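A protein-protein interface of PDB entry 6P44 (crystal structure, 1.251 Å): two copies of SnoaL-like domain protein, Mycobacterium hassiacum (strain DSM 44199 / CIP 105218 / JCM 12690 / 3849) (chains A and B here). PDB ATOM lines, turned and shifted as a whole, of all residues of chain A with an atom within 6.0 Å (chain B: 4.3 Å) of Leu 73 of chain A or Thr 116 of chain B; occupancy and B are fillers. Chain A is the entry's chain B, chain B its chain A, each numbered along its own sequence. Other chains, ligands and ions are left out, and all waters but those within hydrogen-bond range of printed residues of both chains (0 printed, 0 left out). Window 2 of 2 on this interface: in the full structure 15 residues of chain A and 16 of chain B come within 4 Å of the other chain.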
ATOM      1  N   PRO A   4      22.247  18.077 -23.172  1.00  0.00           N
ATOM      2  CA  PRO A   4      22.097  17.424 -24.478  1.00  0.00           C
ATOM      3  C   PRO A   4      20.647  17.107 -24.831  1.00  0.00           C
ATOM      4  O   PRO A   4      20.231  17.313 -25.987  1.00  0.00           O
ATOM      5  CB  PRO A   4      23.001  16.190 -24.340  1.00  0.00           C
ATOM      6  CG  PRO A   4      24.052  16.609 -23.372  1.00  0.00           C
ATOM      7  CD  PRO A   4      23.329  17.471 -22.380  1.00  0.00           C
ATOM      8  N   ARG A  71      22.967  12.811 -32.663  1.00  0.00           N
ATOM      9  CA  ARG A  71      23.877  12.603 -31.541  1.00  0.00           C
ATOM     10  C   ARG A  71      24.067  13.931 -30.820  1.00  0.00           C
ATOM     11  O   ARG A  71      24.764  14.829 -31.323  1.00  0.00           O
ATOM     12  CB  ARG A  71      25.231  12.035 -31.995  1.00  0.00           C
ATOM     13  CG  ARG A  71      25.155  10.640 -32.634  1.00  0.00           C
ATOM     14  CD  ARG A  71      25.281  10.688 -34.124  1.00  0.00           C
ATOM     15  NE  ARG A  71      24.850   9.460 -34.804  1.00  0.00           N
ATOM     16  CZ  ARG A  71      25.635   8.445 -35.174  1.00  0.00           C
ATOM     17  NH1 ARG A  71      26.930   8.449 -34.934  1.00  0.00           N
ATOM     18  NH2 ARG A  71      25.102   7.396 -35.793  1.00  0.00           N
ATOM     19  N   ALA A  72      23.464  14.039 -29.643  1.00  0.00           N
ATOM     20  CA  ALA A  72      23.574  15.213 -28.789  1.00  0.00           C
ATOM     21  C   ALA A  72      24.640  14.933 -27.739  1.00  0.00           C
ATOM     22  O   ALA A  72      24.466  14.059 -26.883  1.00  0.00           O
ATOM     23  CB  ALA A  72      22.225  15.548 -28.160  1.00  0.00           C
ATOM     24  N   LEU A  73      25.739  15.681 -27.815  1.00  0.00           N
ATOM     25  CA  LEU A  73      26.950  15.421 -27.042  1.00  0.00           C
ATOM     26  C   LEU A  73      27.503  16.756 -26.585  1.00  0.00           C
ATOM     27  O   LEU A  73      27.696  17.646 -27.407  1.00  0.00           O
ATOM     28  CB  LEU A  73      28.024  14.756 -27.929  1.00  0.00           C
ATOM     29  CG  LEU A  73      27.586  13.458 -28.588  1.00  0.00           C
ATOM     30  CD1 LEU A  73      28.662  12.970 -29.514  1.00  0.00           C
ATOM     31  CD2 LEU A  73      27.234  12.380 -27.574  1.00  0.00           C
ATOM     32  N   GLY A  74      27.812  16.892 -25.306  1.00  0.00           N
ATOM     33  CA  GLY A  74      28.346  18.167 -24.841  1.00  0.00           C
ATOM     34  C   GLY A  74      27.371  19.276 -25.167  1.00  0.00           C
ATOM     35  O   GLY A  74      26.169  19.172 -24.895  1.00  0.00           O
ATOM     36  N   HIS A  75      27.880  20.346 -25.783  1.00  0.00           N
ATOM     37  CA  HIS A  75      27.070  21.492 -26.184  1.00  0.00           C
ATOM     38  C   HIS A  75      26.664  21.430 -27.650  1.00  0.00           C
ATOM     39  O   HIS A  75      26.225  22.445 -28.214  1.00  0.00           O
ATOM     40  CB  HIS A  75      27.814  22.797 -25.883  1.00  0.00           C
ATOM     41  CG  HIS A  75      28.241  22.917 -24.458  1.00  0.00           C
ATOM     42  ND1 HIS A  75      27.342  23.070 -23.423  1.00  0.00           N
ATOM     43  CD2 HIS A  75      29.467  22.867 -23.886  1.00  0.00           C
ATOM     44  CE1 HIS A  75      27.997  23.128 -22.278  1.00  0.00           C
ATOM     45  NE2 HIS A  75      29.287  23.003 -22.531  1.00  0.00           N
ATOM     46  N   GLU A  76      26.799  20.260 -28.277  1.00  0.00           N
ATOM     47  CA  GLU A  76      26.631  20.119 -29.713  1.00  0.00           C
ATOM     48  C   GLU A  76      25.572  19.071 -30.043  1.00  0.00           C
ATOM     49  O   GLU A  76      25.294  18.161 -29.264  1.00  0.00           O
ATOM     50  CB  GLU A  76      27.951  19.732 -30.395  1.00  0.00           C
ATOM     51  CG  GLU A  76      29.157  20.550 -29.941  1.00  0.00           C
ATOM     52  CD  GLU A  76      30.273  20.609 -30.967  1.00  0.00           C
ATOM     53  OE1 GLU A  76      30.032  20.317 -32.162  1.00  0.00           O
ATOM     54  OE2 GLU A  76      31.393  20.962 -30.563  1.00  0.00           O
ATOM     55  N   VAL A  77      25.033  19.173 -31.254  1.00  0.00           N
ATOM     56  CA  VAL A  77      24.216  18.107 -31.822  1.00  0.00           C
ATOM     57  C   VAL A  77      24.618  17.938 -33.280  1.00  0.00           C
ATOM     58  O   VAL A  77      24.582  18.905 -34.051  1.00  0.00           O
ATOM     59  CB  VAL A  77      22.707  18.398 -31.738  1.00  0.00           C
ATOM     60  CG1 VAL A  77      21.932  17.204 -32.292  1.00  0.00           C
ATOM     61  CG2 VAL A  77      22.261  18.697 -30.310  1.00  0.00           C
ATOM     62  N   ALA A  78      25.011  16.726 -33.655  1.00  0.00           N
ATOM     63  CA  ALA A  78      25.232  16.363 -35.050  1.00  0.00           C
ATOM     64  C   ALA A  78      24.068  15.503 -35.482  1.00  0.00           C
ATOM     65  O   ALA A  78      23.675  14.584 -34.756  1.00  0.00           O
ATOM     66  CB  ALA A  78      26.529  15.583 -35.241  1.00  0.00           C
ATOM     67  N   VAL B  40      32.916  13.949 -29.148  1.00  0.00           N
ATOM     68  CA  VAL B  40      32.530  15.296 -28.750  1.00  0.00           C
ATOM     69  C   VAL B  40      31.922  15.240 -27.363  1.00  0.00           C
ATOM     70  O   VAL B  40      31.165  14.322 -27.038  1.00  0.00           O
ATOM     71  CB  VAL B  40      31.591  15.906 -29.804  1.00  0.00           C
ATOM     72  CG1 VAL B  40      30.975  17.194 -29.336  1.00  0.00           C
ATOM     73  CG2 VAL B  40      32.378  16.168 -31.087  1.00  0.00           C
ATOM     74  N   TYR B 114      31.238  12.170 -33.523  1.00  0.00           N
ATOM     75  CA  TYR B 114      29.940  12.172 -32.858  1.00  0.00           C
ATOM     76  C   TYR B 114      29.382  10.754 -32.914  1.00  0.00           C
ATOM     77  O   TYR B 114      28.902  10.307 -33.961  1.00  0.00           O
ATOM     78  CB  TYR B 114      28.979  13.147 -33.534  1.00  0.00           C
ATOM     79  CG  TYR B 114      29.439  14.596 -33.621  1.00  0.00           C
ATOM     80  CD1 TYR B 114      30.317  15.005 -34.612  1.00  0.00           C
ATOM     81  CD2 TYR B 114      28.947  15.565 -32.749  1.00  0.00           C
ATOM     82  CE1 TYR B 114      30.715  16.296 -34.715  1.00  0.00           C
ATOM     83  CE2 TYR B 114      29.348  16.886 -32.844  1.00  0.00           C
ATOM     84  CZ  TYR B 114      30.243  17.246 -33.830  1.00  0.00           C
ATOM     85  OH  TYR B 114      30.677  18.539 -33.972  1.00  0.00           O
ATOM     86  N   TRP B 115      29.411  10.076 -31.780  1.00  0.00           N
ATOM     87  CA  TRP B 115      28.945   8.704 -31.631  1.00  0.00           C
ATOM     88  C   TRP B 115      28.845   8.444 -30.141  1.00  0.00           C
ATOM     89  O   TRP B 115      29.438   9.172 -29.330  1.00  0.00           O
ATOM     90  CB  TRP B 115      29.921   7.699 -32.263  1.00  0.00           C
ATOM     91  CG  TRP B 115      31.264   7.724 -31.615  1.00  0.00           C
ATOM     92  CD1 TRP B 115      32.286   8.581 -31.888  1.00  0.00           C
ATOM     93  CD2 TRP B 115      31.727   6.879 -30.546  1.00  0.00           C
ATOM     94  NE1 TRP B 115      33.351   8.334 -31.050  1.00  0.00           N
ATOM     95  CE2 TRP B 115      33.036   7.287 -30.225  1.00  0.00           C
ATOM     96  CE3 TRP B 115      31.154   5.827 -29.823  1.00  0.00           C
ATOM     97  CZ2 TRP B 115      33.790   6.671 -29.231  1.00  0.00           C
ATOM     98  CZ3 TRP B 115      31.910   5.220 -28.836  1.00  0.00           C
ATOM     99  CH2 TRP B 115      33.198   5.655 -28.538  1.00  0.00           C
ATOM    100  N   THR B 116      28.089   7.394 -29.795  1.00  0.00           N
ATOM    101  CA  THR B 116      28.022   6.866 -28.437  1.00  0.00           C
ATOM    102  C   THR B 116      27.887   5.358 -28.544  1.00  0.00           C
ATOM    103  O   THR B 116      27.709   4.836 -29.647  1.00  0.00           O
ATOM    104  CB  THR B 116      26.827   7.373 -27.625  1.00  0.00           C
ATOM    105  OG1 THR B 116      25.671   6.622 -27.977  1.00  0.00           O
ATOM    106  CG2 THR B 116      26.549   8.842 -27.835  1.00  0.00           C
ATOM    107  N   PRO B 117      27.911   4.624 -27.427  1.00  0.00           N
ATOM    108  CA  PRO B 117      27.683   3.175 -27.514  1.00  0.00           C
ATOM    109  C   PRO B 117      26.344   2.792 -28.095  1.00  0.00           C
ATOM    110  O   PRO B 117      26.193   1.656 -28.558  1.00  0.00           O
ATOM    111  CB  PRO B 117      27.816   2.709 -26.056  1.00  0.00           C
ATOM    112  CG  PRO B 117      28.750   3.664 -25.456  1.00  0.00           C
ATOM    113  CD  PRO B 117      28.418   4.994 -26.094  1.00  0.00           C
ATOM    114  N   GLU B 118      25.387   3.722 -28.154  1.00  0.00           N
ATOM    115  CA  GLU B 118      24.123   3.455 -28.837  1.00  0.00           C
ATOM    116  C   GLU B 118      24.309   3.254 -30.335  1.00  0.00           C
ATOM    117  O   GLU B 118      23.435   2.675 -30.995  1.00  0.00           O
ATOM    118  CB  GLU B 118      23.154   4.614 -28.606  1.00  0.00           C
ATOM    119  CG  GLU B 118      21.753   4.339 -29.130  1.00  0.00           C
ATOM    120  CD  GLU B 118      20.679   4.781 -28.166  1.00  0.00           C
ATOM    121  OE1 GLU B 118      20.480   6.010 -28.068  1.00  0.00           O
ATOM    122  OE2 GLU B 118      20.046   3.909 -27.505  1.00  0.00           O
ATOM    123  N   ASN B 119      25.422   3.721 -30.887  1.00  0.00           N
ATOM    124  CA  ASN B 119      25.724   3.576 -32.299  1.00  0.00           C
ATOM    125  C   ASN B 119      26.595   2.361 -32.579  1.00  0.00           C
ATOM    126  O   ASN B 119      27.247   2.305 -33.629  1.00  0.00           O
ATOM    127  CB  ASN B 119      26.404   4.846 -32.808  1.00  0.00           C
ATOM    128  CG  ASN B 119      25.643   6.113 -32.425  1.00  0.00           C
ATOM    129  OD1 ASN B 119      26.170   6.983 -31.754  1.00  0.00           O
ATOM    130  ND2 ASN B 119      24.392   6.212 -32.852  1.00  0.00           N
ATOM    131  N   ILE B 120      26.625   1.399 -31.656  1.00  0.00           N
ATOM    132  CA  ILE B 120      27.404   0.175 -31.790  1.00  0.00           C
ATOM    133  C   ILE B 120      26.422  -0.986 -31.879  1.00  0.00           C
ATOM    134  O   ILE B 120      25.578  -1.168 -30.992  1.00  0.00           O
ATOM    135  CB  ILE B 120      28.379   0.005 -30.614  1.00  0.00           C
ATOM    136  CG1 ILE B 120      29.441   1.106 -30.668  1.00  0.00           C
ATOM    137  CG2 ILE B 120      29.020  -1.393 -30.630  1.00  0.00           C
ATOM    138  CD1 ILE B 120      30.426   1.103 -29.512  1.00  0.00           C
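No position is printed for both chains. Of the 10 pairs that touch across the chains among the printed residues, none has its exchanged pair printed and touching as well.
Trp 115 of chain B touches Arg 71 of chain A. Leu 73 of chain A touches Val 40 of chain B (CB to O, 3.3 Å). CD1 of Leu 73 of chain A touches CA of Tyr 114 of chain B (3.7 Å). N of Trp 115 of chain B touches CD1 of Leu 73 of chain A, at 3.8 Å. Leu 73 of chain A touches Thr 116 of chain B. Glu 76 of chain A touches Val 40 of chain B. Tyr 114 of chain B touches Ala 78 of chain A (CD2 to CB, 3.5 Å).
Printed residues of chain A that touch a printed residue of chain B: Arg 71, Leu 73, Glu 76 and Ala 78. Hydrophobic or aromatic side chains of chain A within 4 Å of the printed part of chain B: Leu 73 and Ala 78. Along chain A the printed residues that touch a printed residue of chain B span positions 71 to 78. Printed residues of chain B that touch a printed residue of chain A: Val 40, Tyr 114, Trp 115, Thr 116 and Asn 119. Hydrophobic or aromatic side chains of chain B within 4 Å of the printed part of chain A: Val 40 and Tyr 114. Among the printed residues, 10 pairs touch across the chains.
OG1 of Thr 116 of chain B lies within hydrogen-bond range of N of Glu 118 of chain B (2.9 Å). N of Thr 116 of chain B lies within hydrogen-bond range of OD1 of Asn 119 of chain B. N of Arg 71 of chain A is in hydrogen-bond range of O of Ala 78 of chain A (2.8 Å).
Leu 73 of chain A touches four residues of chain B. Of the printed residues of chain B, Ala 78 of chain A touches Tyr 114 (3.5 Å). Of the printed residues of chain A, Val 40 of chain B touches Leu 73 and Glu 76. Of the printed residues of chain A, Tyr 114 of chain B touches Arg 71 (2.9 Å), Leu 73 (3.7 Å), Glu 76 (2.6 Å) and Ala 78 (3.5 Å). Of the printed residues of chain A, Thr 116 of chain B touches Leu 73. Of the printed residues of chain A, Asn 119 of chain B touches Arg 71. The nearest printed residue of chain B that does not touch Leu 73 of chain A is Asn 119 of chain B (6.9 Å).
The guanidinium group of Arg 71 of chain A sits at hydrogen-bond distance from the backbone carbonyl oxygen of Tyr 114 of chain B (2.9 Å). OH of Tyr 114 of chain B is in hydrogen-bond range of OE1 of Glu 76 of chain A, at 2.6 Å. NH2 of Arg 71 of chain A lies close to ND2 of Asn 119 of chain B (3.2 Å).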
